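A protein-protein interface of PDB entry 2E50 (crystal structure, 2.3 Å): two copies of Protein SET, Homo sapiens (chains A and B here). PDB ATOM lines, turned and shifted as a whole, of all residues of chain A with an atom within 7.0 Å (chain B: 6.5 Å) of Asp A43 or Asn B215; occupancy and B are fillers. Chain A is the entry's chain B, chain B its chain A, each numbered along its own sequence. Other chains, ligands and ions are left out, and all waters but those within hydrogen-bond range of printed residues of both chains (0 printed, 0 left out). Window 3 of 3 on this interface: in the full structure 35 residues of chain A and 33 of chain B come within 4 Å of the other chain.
The side-chain amide nitrogen (NE2) of Gln A39 sits at hydrogen-bond distance from the backbone carbonyl oxygen (O) of Pro B214 (2.8 Å). The guanidinium group of Arg B71 is in hydrogen-bond range of the side-chain amide oxygen of Gln A39 (3.0 Å). ND2 of Asn B215 lies within hydrogen-bond range of OD1 of Asp A43.
The guanidinium group (NH1) of Arg B71 lies within hydrogen-bond range of the backbone carbonyl oxygen (O) of Pro B214, at 3.4 Å. The side-chain amide oxygen (OD1) of Asn B215 lies within hydrogen-bond range of the backbone NH (N) of Leu B217 (2.8 Å). NE2 of Gln A39 is in hydrogen-bond range of OD1 of Asp A43, 3.0 Å away. The backbone carbonyl oxygen (O) of Asn B215 lies close to the side-chain amide oxygen (OE1) of Gln B218, at 3.1 Å. NH2 of Arg B71 lies within hydrogen-bond range of O of Trp B213 (2.7 Å). The backbone carbonyl oxygen (O) of Asp A36 lies close to the side-chain amide nitrogen (ND2) of Asn A40 (3.4 Å).
Asp A36 touches Leu B217 (CA to CD2, 3.5 Å). Gln A39 touches Asn B215. Gln A39 touches Pro B216. Gln A39 touches Leu B217. Ile A42 touches Phe B68. Arg B71 touches Ile A42 (NH1 to CD1, 3.9 Å). Ile A42 touches Pro B214. Pro B214 touches Asn A46 (O to ND2, 3.9 Å).
Of the printed residues of chain B, Asp A36 touches Leu B217. Of the printed residues of chain B, Gln A39 touches Arg B71 (3.0 Å), Pro B214 (2.8 Å), Asn B215 (3.4 Å), Pro B216 (3.9 Å) and Leu B217 (3.7 Å). Of the printed residues of chain B, Ile A42 touches Phe B68 (3.7 Å), Arg B71 (3.9 Å) and Pro B214 (3.5 Å). Of chain B, only Asn B215 comes within 4 Å of Asp A43. Of the printed residues of chain A, Phe B68 touches Ile A42 (3.7 Å). Asn B215 touches just these residues of chain A: Gln A39 and Asp A43. Printed residues of chain A within 4 Å of Leu B217: Asp A36 and Gln A39. The nearest residue of chain A that does not touch Asn B215 is Asn A46 (5.6 Å).
Hydrophobic or aromatic side chains of chain B within 4 Å of the printed part of chain A: Phe B68, Pro B216 and Leu B217. Among the printed residues, no Asp or Glu carboxylate lies within 4 Å of a Lys or Arg side-chain nitrogen of the other chain.
No position is printed for both chains.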
ATOM      1  N   ASP A  36       8.840  13.477   5.066  1.00  0.00           N
ATOM      2  CA  ASP A  36       7.934  12.962   4.041  1.00  0.00           C
ATOM      3  C   ASP A  36       8.647  11.965   3.140  1.00  0.00           C
ATOM      4  O   ASP A  36       8.060  10.988   2.730  1.00  0.00           O
ATOM      5  CB  ASP A  36       7.378  14.120   3.209  1.00  0.00           C
ATOM      6  CG  ASP A  36       6.441  13.645   2.094  1.00  0.00           C
ATOM      7  OD1 ASP A  36       6.891  13.523   0.931  1.00  0.00           O
ATOM      8  OD2 ASP A  36       5.263  13.369   2.392  1.00  0.00           O
ATOM      9  N   VAL A  38      11.446  10.181   3.865  1.00  0.00           N
ATOM     10  CA  VAL A  38      11.875   9.036   4.666  1.00  0.00           C
ATOM     11  C   VAL A  38      10.688   8.094   4.910  1.00  0.00           C
ATOM     12  O   VAL A  38      10.811   6.892   4.756  1.00  0.00           O
ATOM     13  CB  VAL A  38      12.521   9.508   6.002  1.00  0.00           C
ATOM     14  CG1 VAL A  38      12.711   8.392   6.908  1.00  0.00           C
ATOM     15  CG2 VAL A  38      13.867  10.225   5.683  1.00  0.00           C
ATOM     16  N   GLN A  39       9.541   8.688   5.238  1.00  0.00           N
ATOM     17  CA  GLN A  39       8.291   7.971   5.343  1.00  0.00           C
ATOM     18  C   GLN A  39       7.913   7.333   4.037  1.00  0.00           C
ATOM     19  O   GLN A  39       7.370   6.274   4.075  1.00  0.00           O
ATOM     20  CB  GLN A  39       7.149   8.898   5.772  1.00  0.00           C
ATOM     21  CG  GLN A  39       5.926   8.130   6.212  1.00  0.00           C
ATOM     22  CD  GLN A  39       6.215   7.193   7.353  1.00  0.00           C
ATOM     23  OE1 GLN A  39       6.793   7.579   8.370  1.00  0.00           O
ATOM     24  NE2 GLN A  39       5.840   5.945   7.182  1.00  0.00           N
ATOM     25  N   ASN A  40       8.137   7.991   2.888  1.00  0.00           N
ATOM     26  CA  ASN A  40       7.884   7.316   1.619  1.00  0.00           C
ATOM     27  C   ASN A  40       8.680   6.007   1.487  1.00  0.00           C
ATOM     28  O   ASN A  40       8.161   5.038   0.998  1.00  0.00           O
ATOM     29  CB  ASN A  40       8.117   8.242   0.384  1.00  0.00           C
ATOM     30  CG  ASN A  40       6.978   9.240   0.158  1.00  0.00           C
ATOM     31  OD1 ASN A  40       5.842   9.001   0.554  1.00  0.00           O
ATOM     32  ND2 ASN A  40       7.273  10.349  -0.532  1.00  0.00           N
ATOM     33  N   GLU A  41       9.941   6.006   1.909  1.00  0.00           N
ATOM     34  CA  GLU A  41      10.791   4.793   1.947  1.00  0.00           C
ATOM     35  C   GLU A  41      10.277   3.795   2.949  1.00  0.00           C
ATOM     36  O   GLU A  41      10.192   2.624   2.642  1.00  0.00           O
ATOM     37  CB  GLU A  41      12.243   5.122   2.287  1.00  0.00           C
ATOM     38  CG  GLU A  41      12.906   6.107   1.288  1.00  0.00           C
ATOM     39  CD  GLU A  41      13.604   5.422   0.083  1.00  0.00           C
ATOM     40  OE1 GLU A  41      14.671   5.963  -0.357  1.00  0.00           O
ATOM     41  OE2 GLU A  41      13.091   4.370  -0.424  1.00  0.00           O
ATOM     42  N   ILE A  42       9.941   4.254   4.155  1.00  0.00           N
ATOM     43  CA  ILE A  42       9.296   3.381   5.101  1.00  0.00           C
ATOM     44  C   ILE A  42       8.071   2.684   4.492  1.00  0.00           C
ATOM     45  O   ILE A  42       7.955   1.477   4.587  1.00  0.00           O
ATOM     46  CB  ILE A  42       8.935   4.097   6.429  1.00  0.00           C
ATOM     47  CG1 ILE A  42      10.238   4.514   7.158  1.00  0.00           C
ATOM     48  CG2 ILE A  42       8.013   3.196   7.250  1.00  0.00           C
ATOM     49  CD1 ILE A  42      10.103   5.365   8.414  1.00  0.00           C
ATOM     50  N   ASP A  43       7.167   3.460   3.885  1.00  0.00           N
ATOM     51  CA  ASP A  43       5.944   2.935   3.290  1.00  0.00           C
ATOM     52  C   ASP A  43       6.264   1.878   2.235  1.00  0.00           C
ATOM     53  O   ASP A  43       5.628   0.830   2.210  1.00  0.00           O
ATOM     54  CB  ASP A  43       5.074   4.057   2.682  1.00  0.00           C
ATOM     55  CG  ASP A  43       4.419   4.973   3.757  1.00  0.00           C
ATOM     56  OD1 ASP A  43       4.344   4.649   4.974  1.00  0.00           O
ATOM     57  OD2 ASP A  43       3.931   6.031   3.357  1.00  0.00           O
ATOM     58  N   ARG A  44       7.259   2.118   1.397  1.00  0.00           N
ATOM     59  CA  ARG A  44       7.596   1.137   0.353  1.00  0.00           C
ATOM     60  C   ARG A  44       8.090  -0.157   0.962  1.00  0.00           C
ATOM     61  O   ARG A  44       7.795  -1.209   0.460  1.00  0.00           O
ATOM     62  CB  ARG A  44       8.646   1.669  -0.602  1.00  0.00           C
ATOM     63  CG  ARG A  44       8.082   2.640  -1.580  1.00  0.00           C
ATOM     64  CD  ARG A  44       9.125   3.025  -2.635  1.00  0.00           C
ATOM     65  NE  ARG A  44      10.065   4.013  -2.105  1.00  0.00           N
ATOM     66  CZ  ARG A  44       9.928   5.335  -2.242  1.00  0.00           C
ATOM     67  NH1 ARG A  44       8.893   5.846  -2.920  1.00  0.00           N
ATOM     68  NH2 ARG A  44      10.843   6.138  -1.728  1.00  0.00           N
ATOM     69  N   LEU A  45       8.842  -0.050   2.055  1.00  0.00           N
ATOM     70  CA  LEU A  45       9.418  -1.184   2.745  1.00  0.00           C
ATOM     71  C   LEU A  45       8.348  -1.940   3.525  1.00  0.00           C
ATOM     72  O   LEU A  45       8.383  -3.153   3.581  1.00  0.00           O
ATOM     73  CB  LEU A  45      10.583  -0.731   3.673  1.00  0.00           C
ATOM     74  CG  LEU A  45      11.922  -0.335   3.009  1.00  0.00           C
ATOM     75  CD1 LEU A  45      12.944   0.216   4.006  1.00  0.00           C
ATOM     76  CD2 LEU A  45      12.560  -1.448   2.096  1.00  0.00           C
ATOM     77  N   ASN A  46       7.406  -1.228   4.130  1.00  0.00           N
ATOM     78  CA  ASN A  46       6.253  -1.870   4.779  1.00  0.00           C
ATOM     79  C   ASN A  46       5.442  -2.649   3.761  1.00  0.00           C
ATOM     80  O   ASN A  46       5.037  -3.763   4.029  1.00  0.00           O
ATOM     81  CB  ASN A  46       5.328  -0.838   5.438  1.00  0.00           C
ATOM     82  CG  ASN A  46       5.897  -0.256   6.728  1.00  0.00           C
ATOM     83  OD1 ASN A  46       6.806  -0.806   7.325  1.00  0.00           O
ATOM     84  ND2 ASN A  46       5.317   0.852   7.175  1.00  0.00           N
ATOM     85  N   GLU A  47       5.209  -2.046   2.594  1.00  0.00           N
ATOM     86  CA  GLU A  47       4.505  -2.707   1.497  1.00  0.00           C
ATOM     87  C   GLU A  47       5.234  -3.962   0.993  1.00  0.00           C
ATOM     88  O   GLU A  47       4.592  -5.025   0.828  1.00  0.00           O
ATOM     89  CB  GLU A  47       4.248  -1.738   0.339  1.00  0.00           C
ATOM     90  CG  GLU A  47       3.241  -0.637   0.747  1.00  0.00           C
ATOM     91  CD  GLU A  47       3.169   0.587  -0.165  1.00  0.00           C
ATOM     92  OE1 GLU A  47       3.513   0.470  -1.382  1.00  0.00           O
ATOM     93  OE2 GLU A  47       2.722   1.672   0.348  1.00  0.00           O
ATOM     94  N   GLN A  48       6.540  -3.845   0.732  1.00  0.00           N
ATOM     95  CA  GLN A  48       7.320  -4.992   0.271  1.00  0.00           C
ATOM     96  C   GLN A  48       7.278  -6.147   1.301  1.00  0.00           C
ATOM     97  O   GLN A  48       7.082  -7.275   0.926  1.00  0.00           O
ATOM     98  CB  GLN A  48       8.749  -4.622  -0.057  1.00  0.00           C
ATOM     99  CG  GLN A  48       8.874  -3.799  -1.292  1.00  0.00           C
ATOM    100  CD  GLN A  48      10.187  -3.008  -1.437  1.00  0.00           C
ATOM    101  OE1 GLN A  48      10.374  -2.319  -2.433  1.00  0.00           O
ATOM    102  NE2 GLN A  48      11.079  -3.109  -0.484  1.00  0.00           N
ATOM    103  N   ALA A  49       7.427  -5.853   2.579  1.00  0.00           N
ATOM    104  CA  ALA A  49       7.410  -6.898   3.621  1.00  0.00           C
ATOM    105  C   ALA A  49       6.101  -7.658   3.678  1.00  0.00           C
ATOM    106  O   ALA A  49       6.114  -8.871   3.709  1.00  0.00           O
ATOM    107  CB  ALA A  49       7.743  -6.330   4.986  1.00  0.00           C
ATOM    108  N   PHE B  68      13.653   4.624  10.291  1.00  0.00           N
ATOM    109  CA  PHE B  68      12.901   5.024  11.507  1.00  0.00           C
ATOM    110  C   PHE B  68      13.797   5.827  12.413  1.00  0.00           C
ATOM    111  O   PHE B  68      13.321   6.798  12.987  1.00  0.00           O
ATOM    112  CB  PHE B  68      12.326   3.818  12.289  1.00  0.00           C
ATOM    113  CG  PHE B  68      11.091   3.223  11.705  1.00  0.00           C
ATOM    114  CD1 PHE B  68      11.137   2.398  10.569  1.00  0.00           C
ATOM    115  CD2 PHE B  68       9.857   3.490  12.274  1.00  0.00           C
ATOM    116  CE1 PHE B  68       9.949   1.791  10.040  1.00  0.00           C
ATOM    117  CE2 PHE B  68       8.672   2.904  11.781  1.00  0.00           C
ATOM    118  CZ  PHE B  68       8.711   2.053  10.656  1.00  0.00           C
ATOM    119  N   ARG B  71      13.951   9.183  10.857  1.00  0.00           N
ATOM    120  CA  ARG B  71      12.648   9.837  11.029  1.00  0.00           C
ATOM    121  C   ARG B  71      12.486  10.460  12.407  1.00  0.00           C
ATOM    122  O   ARG B  71      12.033  11.615  12.523  1.00  0.00           O
ATOM    123  CB  ARG B  71      11.495   8.858  10.742  1.00  0.00           C
ATOM    124  CG  ARG B  71      10.138   9.547  10.630  1.00  0.00           C
ATOM    125  CD  ARG B  71       9.016   8.538  10.579  1.00  0.00           C
ATOM    126  NE  ARG B  71       8.784   7.877  11.874  1.00  0.00           N
ATOM    127  CZ  ARG B  71       7.951   6.847  12.049  1.00  0.00           C
ATOM    128  NH1 ARG B  71       7.310   6.322  11.021  1.00  0.00           N
ATOM    129  NH2 ARG B  71       7.813   6.292  13.240  1.00  0.00           N
ATOM    130  N   THR B  85       0.004  15.180  15.800  1.00  0.00           N
ATOM    131  CA  THR B  85      -0.268  13.796  15.406  1.00  0.00           C
ATOM    132  C   THR B  85      -1.362  13.164  16.295  1.00  0.00           C
ATOM    133  O   THR B  85      -2.327  12.612  15.773  1.00  0.00           O
ATOM    134  CB  THR B  85       1.056  12.958  15.381  1.00  0.00           C
ATOM    135  OG1 THR B  85       1.958  13.556  14.448  1.00  0.00           O
ATOM    136  CG2 THR B  85       0.826  11.497  14.943  1.00  0.00           C
ATOM    137  N   ASP B 211      -0.848   1.648  14.721  1.00  0.00           N
ATOM    138  CA  ASP B 211      -1.522   2.626  13.872  1.00  0.00           C
ATOM    139  C   ASP B 211      -0.559   3.738  13.520  1.00  0.00           C
ATOM    140  O   ASP B 211      -0.247   3.978  12.349  1.00  0.00           O
ATOM    141  CB  ASP B 211      -2.626   3.257  14.705  1.00  0.00           C
ATOM    142  CG  ASP B 211      -3.894   3.474  13.945  1.00  0.00           C
ATOM    143  OD1 ASP B 211      -4.932   2.958  14.437  1.00  0.00           O
ATOM    144  OD2 ASP B 211      -3.862   4.164  12.890  1.00  0.00           O
ATOM    145  N   ILE B 212      -0.093   4.423  14.557  1.00  0.00           N
ATOM    146  CA  ILE B 212       0.623   5.680  14.420  1.00  0.00           C
ATOM    147  C   ILE B 212       2.115   5.497  14.141  1.00  0.00           C
ATOM    148  O   ILE B 212       2.648   6.133  13.230  1.00  0.00           O
ATOM    149  CB  ILE B 212       0.451   6.568  15.679  1.00  0.00           C
ATOM    150  CG1 ILE B 212      -1.028   6.948  15.874  1.00  0.00           C
ATOM    151  CG2 ILE B 212       1.287   7.801  15.515  1.00  0.00           C
ATOM    152  CD1 ILE B 212      -1.306   7.581  17.174  1.00  0.00           C
ATOM    153  N   TRP B 213       2.772   4.628  14.902  1.00  0.00           N
ATOM    154  CA  TRP B 213       4.214   4.423  14.710  1.00  0.00           C
ATOM    155  C   TRP B 213       4.693   4.139  13.268  1.00  0.00           C
ATOM    156  O   TRP B 213       5.653   4.750  12.854  1.00  0.00           O
ATOM    157  CB  TRP B 213       4.769   3.360  15.658  1.00  0.00           C
ATOM    158  CG  TRP B 213       6.235   3.341  15.658  1.00  0.00           C
ATOM    159  CD1 TRP B 213       7.037   2.355  15.184  1.00  0.00           C
ATOM    160  CD2 TRP B 213       7.098   4.382  16.124  1.00  0.00           C
ATOM    161  NE1 TRP B 213       8.326   2.700  15.349  1.00  0.00           N
ATOM    162  CE2 TRP B 213       8.400   3.944  15.920  1.00  0.00           C
ATOM    163  CE3 TRP B 213       6.879   5.659  16.699  1.00  0.00           C
ATOM    164  CZ2 TRP B 213       9.519   4.719  16.253  1.00  0.00           C
ATOM    165  CZ3 TRP B 213       7.985   6.419  17.049  1.00  0.00           C
ATOM    166  CH2 TRP B 213       9.288   5.953  16.803  1.00  0.00           C
ATOM    167  N   PRO B 214       4.060   3.188  12.537  1.00  0.00           N
ATOM    168  CA  PRO B 214       4.546   2.914  11.180  1.00  0.00           C
ATOM    169  C   PRO B 214       4.519   4.129  10.232  1.00  0.00           C
ATOM    170  O   PRO B 214       5.288   4.160   9.277  1.00  0.00           O
ATOM    171  CB  PRO B 214       3.548   1.852  10.629  1.00  0.00           C
ATOM    172  CG  PRO B 214       2.935   1.205  11.869  1.00  0.00           C
ATOM    173  CD  PRO B 214       2.894   2.335  12.896  1.00  0.00           C
ATOM    174  N   ASN B 215       3.591   5.054  10.480  1.00  0.00           N
ATOM    175  CA  ASN B 215       3.411   6.270   9.709  1.00  0.00           C
ATOM    176  C   ASN B 215       2.659   7.337  10.517  1.00  0.00           C
ATOM    177  O   ASN B 215       1.448   7.417  10.442  1.00  0.00           O
ATOM    178  CB  ASN B 215       2.683   6.004   8.384  1.00  0.00           C
ATOM    179  CG  ASN B 215       2.695   7.227   7.480  1.00  0.00           C
ATOM    180  OD1 ASN B 215       2.878   8.359   7.956  1.00  0.00           O
ATOM    181  ND2 ASN B 215       2.502   7.019   6.180  1.00  0.00           N
ATOM    182  N   PRO B 216       3.375   8.140  11.334  1.00  0.00           N
ATOM    183  CA  PRO B 216       2.657   9.202  12.060  1.00  0.00           C
ATOM    184  C   PRO B 216       2.253  10.373  11.155  1.00  0.00           C
ATOM    185  O   PRO B 216       1.435  11.231  11.544  1.00  0.00           O
ATOM    186  CB  PRO B 216       3.668   9.645  13.101  1.00  0.00           C
ATOM    187  CG  PRO B 216       5.038   9.304  12.492  1.00  0.00           C
ATOM    188  CD  PRO B 216       4.812   8.068  11.688  1.00  0.00           C
ATOM    189  N   LEU B 217       2.784  10.372   9.936  1.00  0.00           N
ATOM    190  CA  LEU B 217       2.793  11.558   9.107  1.00  0.00           C
ATOM    191  C   LEU B 217       1.430  11.705   8.487  1.00  0.00           C
ATOM    192  O   LEU B 217       0.980  12.806   8.233  1.00  0.00           O
ATOM    193  CB  LEU B 217       3.915  11.475   8.076  1.00  0.00           C
ATOM    194  CG  LEU B 217       4.143  12.544   7.013  1.00  0.00           C
ATOM    195  CD1 LEU B 217       4.427  13.960   7.631  1.00  0.00           C
ATOM    196  CD2 LEU B 217       5.266  12.065   6.094  1.00  0.00           C
ATOM    197  N   GLN B 218       0.728  10.598   8.316  1.00  0.00           N
ATOM    198  CA  GLN B 218      -0.654  10.666   7.859  1.00  0.00           C
ATOM    199  C   GLN B 218      -1.611  11.310   8.879  1.00  0.00           C
ATOM    200  O   GLN B 218      -2.737  11.674   8.538  1.00  0.00           O
ATOM    201  CB  GLN B 218      -1.149   9.274   7.525  1.00  0.00           C
ATOM    202  CG  GLN B 218      -1.442   8.487   8.740  1.00  0.00           C
ATOM    203  CD  GLN B 218      -1.590   7.013   8.500  1.00  0.00           C
ATOM    204  OE1 GLN B 218      -1.145   6.217   9.329  1.00  0.00           O
ATOM    205  NE2 GLN B 218      -2.219   6.626   7.386  1.00  0.00           N
ATOM    206  N   TYR B 219      -1.205  11.408  10.137  1.00  0.00           N
ATOM    207  CA  TYR B 219      -2.061  12.069  11.101  1.00  0.00           C
ATOM    208  C   TYR B 219      -1.591  13.501  11.267  1.00  0.00           C
ATOM    209  O   TYR B 219      -2.395  14.392  11.462  1.00  0.00           O
ATOM    210  CB  TYR B 219      -2.103  11.314  12.440  1.00  0.00           C
ATOM    211  CG  TYR B 219      -2.705   9.946  12.278  1.00  0.00           C
ATOM    212  CD1 TYR B 219      -1.912   8.800  12.318  1.00  0.00           C
ATOM    213  CD2 TYR B 219      -4.059   9.802  11.998  1.00  0.00           C
ATOM    214  CE1 TYR B 219      -2.462   7.542  12.126  1.00  0.00           C
ATOM    215  CE2 TYR B 219      -4.619   8.551  11.801  1.00  0.00           C
ATOM    216  CZ  TYR B 219      -3.815   7.422  11.880  1.00  0.00           C
ATOM    217  OH  TYR B 219      -4.402   6.190  11.689  1.00  0.00           O
